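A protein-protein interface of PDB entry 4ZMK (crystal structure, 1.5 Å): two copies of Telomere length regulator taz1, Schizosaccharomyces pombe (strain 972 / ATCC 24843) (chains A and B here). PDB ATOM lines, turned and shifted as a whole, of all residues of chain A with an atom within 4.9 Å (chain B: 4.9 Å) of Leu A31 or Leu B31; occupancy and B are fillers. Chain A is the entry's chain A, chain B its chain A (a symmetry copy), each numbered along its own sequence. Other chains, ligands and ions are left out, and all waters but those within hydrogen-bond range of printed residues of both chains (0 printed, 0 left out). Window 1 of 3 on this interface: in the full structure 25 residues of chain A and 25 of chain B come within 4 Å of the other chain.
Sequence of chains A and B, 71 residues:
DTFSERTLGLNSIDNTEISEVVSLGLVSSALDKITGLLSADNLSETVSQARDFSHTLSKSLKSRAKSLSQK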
ATOM      1  N   VAL A  27     -21.526  18.516   5.564  1.00  0.00           N
ATOM      2  CA  VAL A  27     -20.244  17.867   5.301  1.00  0.00           C
ATOM      3  C   VAL A  27     -19.531  17.540   6.610  1.00  0.00           C
ATOM      4  O   VAL A  27     -19.075  16.415   6.811  1.00  0.00           O
ATOM      5  CB  VAL A  27     -19.362  18.744   4.409  1.00  0.00           C
ATOM      6  CG1 VAL A  27     -18.058  18.055   4.122  1.00  0.00           C
ATOM      7  CG2 VAL A  27     -20.094  19.037   3.118  1.00  0.00           C
ATOM      8  N   SER A  28     -19.454  18.526   7.496  1.00  0.00           N
ATOM      9  CA  SER A  28     -18.890  18.353   8.829  1.00  0.00           C
ATOM     10  C   SER A  28     -19.497  17.149   9.545  1.00  0.00           C
ATOM     11  O   SER A  28     -18.791  16.334  10.120  1.00  0.00           O
ATOM     12  CB  SER A  28     -19.117  19.627   9.655  1.00  0.00           C
ATOM     13  OG  SER A  28     -18.544  19.534  10.946  1.00  0.00           O
ATOM     14  N   SER A  29     -20.823  17.072   9.514  1.00  0.00           N
ATOM     15  CA  SER A  29     -21.560  15.988  10.147  1.00  0.00           C
ATOM     16  C   SER A  29     -21.168  14.637   9.545  1.00  0.00           C
ATOM     17  O   SER A  29     -20.963  13.664  10.264  1.00  0.00           O
ATOM     18  CB  SER A  29     -23.064  16.228  10.001  1.00  0.00           C
ATOM     19  OG  SER A  29     -23.807  15.181  10.586  1.00  0.00           O
ATOM     20  N   ALA A  30     -21.077  14.594   8.219  1.00  0.00           N
ATOM     21  CA  ALA A  30     -20.696  13.381   7.512  1.00  0.00           C
ATOM     22  C   ALA A  30     -19.265  12.975   7.854  1.00  0.00           C
ATOM     23  O   ALA A  30     -19.002  11.809   8.152  1.00  0.00           O
ATOM     24  CB  ALA A  30     -20.863  13.563   6.008  1.00  0.00           C
ATOM     25  N   LEU A  31     -18.350  13.936   7.848  1.00  0.00           N
ATOM     26  CA  LEU A  31     -16.962  13.654   8.225  1.00  0.00           C
ATOM     27  C   LEU A  31     -16.811  13.165   9.668  1.00  0.00           C
ATOM     28  O   LEU A  31     -15.966  12.327   9.962  1.00  0.00           O
ATOM     29  CB  LEU A  31     -16.097  14.890   8.020  1.00  0.00           C
ATOM     30  CG  LEU A  31     -15.765  15.241   6.583  1.00  0.00           C
ATOM     31  CD1 LEU A  31     -15.233  16.665   6.521  1.00  0.00           C
ATOM     32  CD2 LEU A  31     -14.739  14.264   6.053  1.00  0.00           C
ATOM     33  N   ASP A  32     -17.612  13.705  10.575  1.00  0.00           N
ATOM     34  CA  ASP A  32     -17.564  13.271  11.971  1.00  0.00           C
ATOM     35  C   ASP A  32     -18.007  11.807  12.128  1.00  0.00           C
ATOM     36  O   ASP A  32     -17.518  11.093  13.000  1.00  0.00           O
ATOM     37  CB  ASP A  32     -18.446  14.170  12.851  1.00  0.00           C
ATOM     38  CG  ASP A  32     -17.880  15.570  13.018  1.00  0.00           C
ATOM     39  OD1 ASP A  32     -16.725  15.800  12.601  1.00  0.00           O
ATOM     40  OD2 ASP A  32     -18.586  16.439  13.582  1.00  0.00           O
ATOM     41  N   LYS A  33     -18.955  11.379  11.299  1.00  0.00           N
ATOM     42  CA  LYS A  33     -19.389   9.991  11.289  1.00  0.00           C
ATOM     43  C   LYS A  33     -18.288   9.076  10.728  1.00  0.00           C
ATOM     44  O   LYS A  33     -18.123   7.955  11.188  1.00  0.00           O
ATOM     45  CB  LYS A  33     -20.684   9.850  10.492  1.00  0.00           C
ATOM     46  CG  LYS A  33     -21.831  10.656  11.097  1.00  0.00           C
ATOM     47  CD  LYS A  33     -23.092  10.592  10.253  1.00  0.00           C
ATOM     48  CE  LYS A  33     -24.261  11.276  10.960  1.00  0.00           C
ATOM     49  NZ  LYS A  33     -25.532  11.168  10.184  1.00  0.00           N
ATOM     50  N   ILE A  34     -17.539   9.567   9.746  1.00  0.00           N
ATOM     51  CA  ILE A  34     -16.365   8.859   9.230  1.00  0.00           C
ATOM     52  C   ILE A  34     -15.272   8.744  10.295  1.00  0.00           C
ATOM     53  O   ILE A  34     -14.696   7.679  10.492  1.00  0.00           O
ATOM     54  CB  ILE A  34     -15.797   9.575   7.974  1.00  0.00           C
ATOM     55  CG1 ILE A  34     -16.770   9.441   6.812  1.00  0.00           C
ATOM     56  CG2 ILE A  34     -14.432   9.034   7.576  1.00  0.00           C
ATOM     57  CD1 ILE A  34     -16.417  10.334   5.648  1.00  0.00           C
ATOM     58  N   THR A  35     -14.983   9.852  10.968  1.00  0.00           N
ATOM     59  CA  THR A  35     -14.042   9.851  12.086  1.00  0.00           C
ATOM     60  C   THR A  35     -14.455   8.842  13.152  1.00  0.00           C
ATOM     61  O   THR A  35     -13.629   8.100  13.679  1.00  0.00           O
ATOM     62  CB  THR A  35     -13.932  11.246  12.725  1.00  0.00           C
ATOM     63  OG1 THR A  35     -13.501  12.179  11.738  1.00  0.00           O
ATOM     64  CG2 THR A  35     -12.930  11.250  13.855  1.00  0.00           C
ATOM     65  N   SER A  54     -16.898   8.187   2.611  1.00  0.00           N
ATOM     66  CA  SER A  54     -15.983   9.185   2.068  1.00  0.00           C
ATOM     67  C   SER A  54     -16.223   9.427   0.583  1.00  0.00           C
ATOM     68  O   SER A  54     -16.315  10.557   0.128  1.00  0.00           O
ATOM     69  CB  SER A  54     -14.537   8.745   2.302  1.00  0.00           C
ATOM     70  OG  SER A  54     -13.621   9.724   1.850  1.00  0.00           O
ATOM     71  N   LEU A  57     -19.654  11.044  -0.156  1.00  0.00           N
ATOM     72  CA  LEU A  57     -19.590  12.454   0.169  1.00  0.00           C
ATOM     73  C   LEU A  57     -18.835  13.232  -0.918  1.00  0.00           C
ATOM     74  O   LEU A  57     -19.286  14.282  -1.374  1.00  0.00           O
ATOM     75  CB  LEU A  57     -18.934  12.638   1.530  1.00  0.00           C
ATOM     76  CG  LEU A  57     -18.772  14.051   2.078  1.00  0.00           C
ATOM     77  CD1 LEU A  57     -20.104  14.681   2.289  1.00  0.00           C
ATOM     78  CD2 LEU A  57     -18.025  14.000   3.390  1.00  0.00           C
ATOM     79  N   SER A  58     -17.696  12.700  -1.345  1.00  0.00           N
ATOM     80  CA  SER A  58     -16.888  13.337  -2.384  1.00  0.00           C
ATOM     81  C   SER A  58     -17.708  13.495  -3.674  1.00  0.00           C
ATOM     82  O   SER A  58     -17.743  14.550  -4.289  1.00  0.00           O
ATOM     83  CB  SER A  58     -15.633  12.518  -2.641  1.00  0.00           C
ATOM     84  OG  SER A  58     -14.744  13.185  -3.504  1.00  0.00           O
ATOM     85  N   LEU A  61     -20.235  16.242  -3.373  1.00  0.00           N
ATOM     86  CA  LEU A  61     -19.671  17.592  -3.398  1.00  0.00           C
ATOM     87  C   LEU A  61     -19.265  17.994  -4.825  1.00  0.00           C
ATOM     88  O   LEU A  61     -19.342  19.160  -5.209  1.00  0.00           O
ATOM     89  CB  LEU A  61     -18.494  17.686  -2.425  1.00  0.00           C
ATOM     90  CG  LEU A  61     -18.921  17.526  -0.956  1.00  0.00           C
ATOM     91  CD1 LEU A  61     -17.802  17.866  -0.017  1.00  0.00           C
ATOM     92  CD2 LEU A  61     -20.127  18.414  -0.672  1.00  0.00           C
ATOM     93  N   VAL B  27     -12.033  20.198  -0.686  1.00  0.00           N
ATOM     94  CA  VAL B  27     -12.641  19.164   0.147  1.00  0.00           C
ATOM     95  C   VAL B  27     -12.692  17.835  -0.602  1.00  0.00           C
ATOM     96  O   VAL B  27     -12.285  16.801  -0.074  1.00  0.00           O
ATOM     97  CB  VAL B  27     -14.043  19.583   0.600  1.00  0.00           C
ATOM     98  CG1 VAL B  27     -14.647  18.525   1.478  1.00  0.00           C
ATOM     99  CG2 VAL B  27     -13.952  20.894   1.349  1.00  0.00           C
ATOM    100  N   SER B  28     -13.181  17.878  -1.837  1.00  0.00           N
ATOM    101  CA  SER B  28     -13.213  16.718  -2.718  1.00  0.00           C
ATOM    102  C   SER B  28     -11.850  16.033  -2.796  1.00  0.00           C
ATOM    103  O   SER B  28     -11.745  14.821  -2.685  1.00  0.00           O
ATOM    104  CB  SER B  28     -13.666  17.147  -4.121  1.00  0.00           C
ATOM    105  OG  SER B  28     -13.764  16.049  -5.009  1.00  0.00           O
ATOM    106  N   SER B  29     -10.815  16.838  -3.011  1.00  0.00           N
ATOM    107  CA  SER B  29      -9.449  16.347  -3.112  1.00  0.00           C
ATOM    108  C   SER B  29      -9.021  15.652  -1.817  1.00  0.00           C
ATOM    109  O   SER B  29      -8.412  14.587  -1.847  1.00  0.00           O
ATOM    110  CB  SER B  29      -8.503  17.505  -3.438  1.00  0.00           C
ATOM    111  OG  SER B  29      -7.165  17.064  -3.520  1.00  0.00           O
ATOM    112  N   ALA B  30      -9.344  16.273  -0.687  1.00  0.00           N
ATOM    113  CA  ALA B  30      -9.018  15.719   0.618  1.00  0.00           C
ATOM    114  C   ALA B  30      -9.762  14.408   0.857  1.00  0.00           C
ATOM    115  O   ALA B  30      -9.164  13.421   1.287  1.00  0.00           O
ATOM    116  CB  ALA B  30      -9.326  16.726   1.720  1.00  0.00           C
ATOM    117  N   LEU B  31     -11.053  14.384   0.546  1.00  0.00           N
ATOM    118  CA  LEU B  31     -11.835  13.152   0.681  1.00  0.00           C
ATOM    119  C   LEU B  31     -11.335  12.014  -0.211  1.00  0.00           C
ATOM    120  O   LEU B  31     -11.380  10.850   0.171  1.00  0.00           O
ATOM    121  CB  LEU B  31     -13.303  13.422   0.376  1.00  0.00           C
ATOM    122  CG  LEU B  31     -14.077  14.176   1.439  1.00  0.00           C
ATOM    123  CD1 LEU B  31     -15.381  14.687   0.847  1.00  0.00           C
ATOM    124  CD2 LEU B  31     -14.344  13.258   2.611  1.00  0.00           C
ATOM    125  N   ASP B  32     -10.881  12.342  -1.412  1.00  0.00           N
ATOM    126  CA  ASP B  32     -10.348  11.323  -2.317  1.00  0.00           C
ATOM    127  C   ASP B  32      -9.065  10.685  -1.763  1.00  0.00           C
ATOM    128  O   ASP B  32      -8.798   9.508  -1.995  1.00  0.00           O
ATOM    129  CB  ASP B  32     -10.065  11.922  -3.704  1.00  0.00           C
ATOM    130  CG  ASP B  32     -11.333  12.275  -4.464  1.00  0.00           C
ATOM    131  OD1 ASP B  32     -12.430  11.903  -3.998  1.00  0.00           O
ATOM    132  OD2 ASP B  32     -11.230  12.914  -5.537  1.00  0.00           O
ATOM    133  N   LYS B  33      -8.262  11.475  -1.056  1.00  0.00           N
ATOM    134  CA  LYS B  33      -7.068  10.963  -0.404  1.00  0.00           C
ATOM    135  C   LYS B  33      -7.438  10.050   0.776  1.00  0.00           C
ATOM    136  O   LYS B  33      -6.759   9.063   1.029  1.00  0.00           O
ATOM    137  CB  LYS B  33      -6.178  12.119   0.050  1.00  0.00           C
ATOM    138  CG  LYS B  33      -5.697  12.976  -1.118  1.00  0.00           C
ATOM    139  CD  LYS B  33      -4.892  14.179  -0.659  1.00  0.00           C
ATOM    140  CE  LYS B  33      -4.295  14.927  -1.850  1.00  0.00           C
ATOM    141  NZ  LYS B  33      -3.440  16.076  -1.426  1.00  0.00           N
ATOM    142  N   ILE B  34      -8.515  10.379   1.480  1.00  0.00           N
ATOM    143  CA  ILE B  34      -9.060   9.514   2.529  1.00  0.00           C
ATOM    144  C   ILE B  34      -9.580   8.197   1.947  1.00  0.00           C
ATOM    145  O   ILE B  34      -9.301   7.124   2.474  1.00  0.00           O
ATOM    146  CB  ILE B  34     -10.201  10.232   3.300  1.00  0.00           C
ATOM    147  CG1 ILE B  34      -9.634  11.383   4.117  1.00  0.00           C
ATOM    148  CG2 ILE B  34     -10.968   9.279   4.203  1.00  0.00           C
ATOM    149  CD1 ILE B  34     -10.706  12.288   4.673  1.00  0.00           C
ATOM    150  N   THR B  35     -10.349   8.289   0.869  1.00  0.00           N
ATOM    151  CA  THR B  35     -10.816   7.105   0.152  1.00  0.00           C
ATOM    152  C   THR B  35      -9.647   6.223  -0.275  1.00  0.00           C
ATOM    153  O   THR B  35      -9.689   5.002  -0.138  1.00  0.00           O
ATOM    154  CB  THR B  35     -11.638   7.490  -1.090  1.00  0.00           C
ATOM    155  OG1 THR B  35     -12.756   8.275  -0.684  1.00  0.00           O
ATOM    156  CG2 THR B  35     -12.151   6.264  -1.806  1.00  0.00           C
ATOM    157  N   SER B  54      -9.643  12.979   8.202  1.00  0.00           N
ATOM    158  CA  SER B  54     -11.071  13.261   8.312  1.00  0.00           C
ATOM    159  C   SER B  54     -11.358  14.338   9.351  1.00  0.00           C
ATOM    160  O   SER B  54     -12.095  15.280   9.105  1.00  0.00           O
ATOM    161  CB  SER B  54     -11.828  11.979   8.660  1.00  0.00           C
ATOM    162  OG  SER B  54     -13.225  12.202   8.707  1.00  0.00           O
ATOM    163  N   LEU B  57      -9.960  17.805   8.371  1.00  0.00           N
ATOM    164  CA  LEU B  57     -10.824  18.395   7.369  1.00  0.00           C
ATOM    165  C   LEU B  57     -12.109  18.941   8.009  1.00  0.00           C
ATOM    166  O   LEU B  57     -12.526  20.064   7.729  1.00  0.00           O
ATOM    167  CB  LEU B  57     -11.142  17.366   6.294  1.00  0.00           C
ATOM    168  CG  LEU B  57     -12.033  17.777   5.129  1.00  0.00           C
ATOM    169  CD1 LEU B  57     -11.386  18.861   4.339  1.00  0.00           C
ATOM    170  CD2 LEU B  57     -12.283  16.583   4.238  1.00  0.00           C
ATOM    171  N   SER B  58     -12.718  18.150   8.884  1.00  0.00           N
ATOM    172  CA  SER B  58     -13.944  18.557   9.569  1.00  0.00           C
ATOM    173  C   SER B  58     -13.702  19.847  10.369  1.00  0.00           C
ATOM    174  O   SER B  58     -14.469  20.796  10.306  1.00  0.00           O
ATOM    175  CB  SER B  58     -14.424  17.440  10.481  1.00  0.00           C
ATOM    176  OG  SER B  58     -15.692  17.720  11.024  1.00  0.00           O
ATOM    177  N   LEU B  61     -13.470  22.837   8.127  1.00  0.00           N
ATOM    178  CA  LEU B  61     -14.744  23.265   7.551  1.00  0.00           C
ATOM    179  C   LEU B  61     -15.604  23.997   8.595  1.00  0.00           C
ATOM    180  O   LEU B  61     -16.360  24.913   8.275  1.00  0.00           O
ATOM    181  CB  LEU B  61     -15.479  22.063   6.953  1.00  0.00           C
ATOM    182  CG  LEU B  61     -14.747  21.460   5.742  1.00  0.00           C
ATOM    183  CD1 LEU B  61     -15.599  20.454   5.029  1.00  0.00           C
ATOM    184  CD2 LEU B  61     -14.340  22.572   4.781  1.00  0.00           C
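The side-chain hydroxyl (OG) of Ser A28 lies within hydrogen-bond range of the side-chain hydroxyl (OG) of Ser B58.
OG of Ser B54 sits at hydrogen-bond distance from O of Leu A31, at 3.0 Å.
The side-chain carboxylate (OD1) of Asp A32 lies within hydrogen-bond range of the side-chain hydroxyl (OG) of Ser B58 (2.7 Å).
The side-chain hydroxyl (OG) of Ser B54 is in hydrogen-bond range of the side-chain hydroxyl (OG1) of Thr A35, 3.0 Å away.
The side-chain hydroxyl of Ser A54 sits at hydrogen-bond distance from the backbone carbonyl oxygen of Leu B31 (3.0 Å).
OG1 of Thr B35 sits at hydrogen-bond distance from OG of Ser A54.
The side-chain hydroxyl (OG) of Ser A58 sits at hydrogen-bond distance from the side-chain hydroxyl (OG) of Ser B28 (3.4 Å).
The side-chain hydroxyl (OG) of Ser A58 sits at hydrogen-bond distance from the side-chain carboxylate (OD1) of Asp B32, 2.7 Å away.
The backbone carbonyl oxygen (O) of Leu A31 sits at hydrogen-bond distance from the side-chain hydroxyl (OG1) of Thr A35 (3.0 Å).
The backbone carbonyl oxygen (O) of Leu B31 is in hydrogen-bond range of the side-chain hydroxyl (OG1) of Thr B35 (3.0 Å).
Of the printed residues of chain B, Leu A31 touches Leu B31 (3.6 Å), Ser B54 (3.0 Å), Leu B57 (3.7 Å) and Ser B58 (3.8 Å).
Of the printed residues of chain B, Ser A54 touches Leu B31 (3.0 Å), Ile B34 (3.6 Å) and Thr B35 (3.0 Å).
Of the printed residues of chain A, Leu B31 touches Leu A31 (3.6 Å), Ser A54 (3.0 Å), Leu A57 (3.7 Å) and Ser A58 (3.8 Å).
Of the printed residues of chain A, Ile B34 touches Ser A54 (3.6 Å).
The nearest printed residue of chain A that does not touch Leu B31 is Leu A61 (4.1 Å).
The nearest printed residue of chain B that does not touch Ser A54 is Asp B32 (5.0 Å).
Of the 13 printed residues of chain A, 10 touch a printed residue of chain B.
Hydrophobic or aromatic side chains of chain A within 4 Å of the printed part of chain B: Val A27, Leu A31, Ile A34, Leu A57 and Leu A61.
Of the 13 printed residues of chain B, 10 touch a printed residue of chain A.
Hydrophobic or aromatic side chains of chain B that line the printed part of chain A: Val B27, Leu B31, Ile B34, Leu B57 and Leu B61.
Among the printed residues, no Asp or Glu carboxylate lies within 4 Å of a Lys or Arg side-chain nitrogen of the other chain.
Ser A28 touches Ser B58, and with the chains exchanged Ser A58 touches Ser B28.
Leu A31 touches its own counterpart, Leu B31.
Leu A31 touches Ser B58, and with the chains exchanged Ser A58 touches Leu B31.
Thr A35 touches Ser B54, and with the chains exchanged Ser A54 touches Thr B35.
Positions printed for both chains: 27, 28, 29, 30, 31, 32, 33, 34, 35, 54, 57, 58 and 61.
CD1 of Leu B61 touches CG1 of Val A27 (3.6 Å).
Leu B31 touches Leu A31 (CD2 to CD2, 3.6 Å).
Leu A31 touches Leu B57 (CD1 to CG, 3.7 Å).
CD1 of Leu A31 touches N of Ser B58, 3.8 Å away.
OG of Ser B54 touches CG2 of Ile A34, at 3.6 Å.
OG of Ser A54 touches CG2 of Ile B34, 3.6 Å away.
CD1 of Leu B31 touches CG of Leu A57, 3.7 Å away.
Leu B31 touches Ser A58.
Leu A61 touches Val B27.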
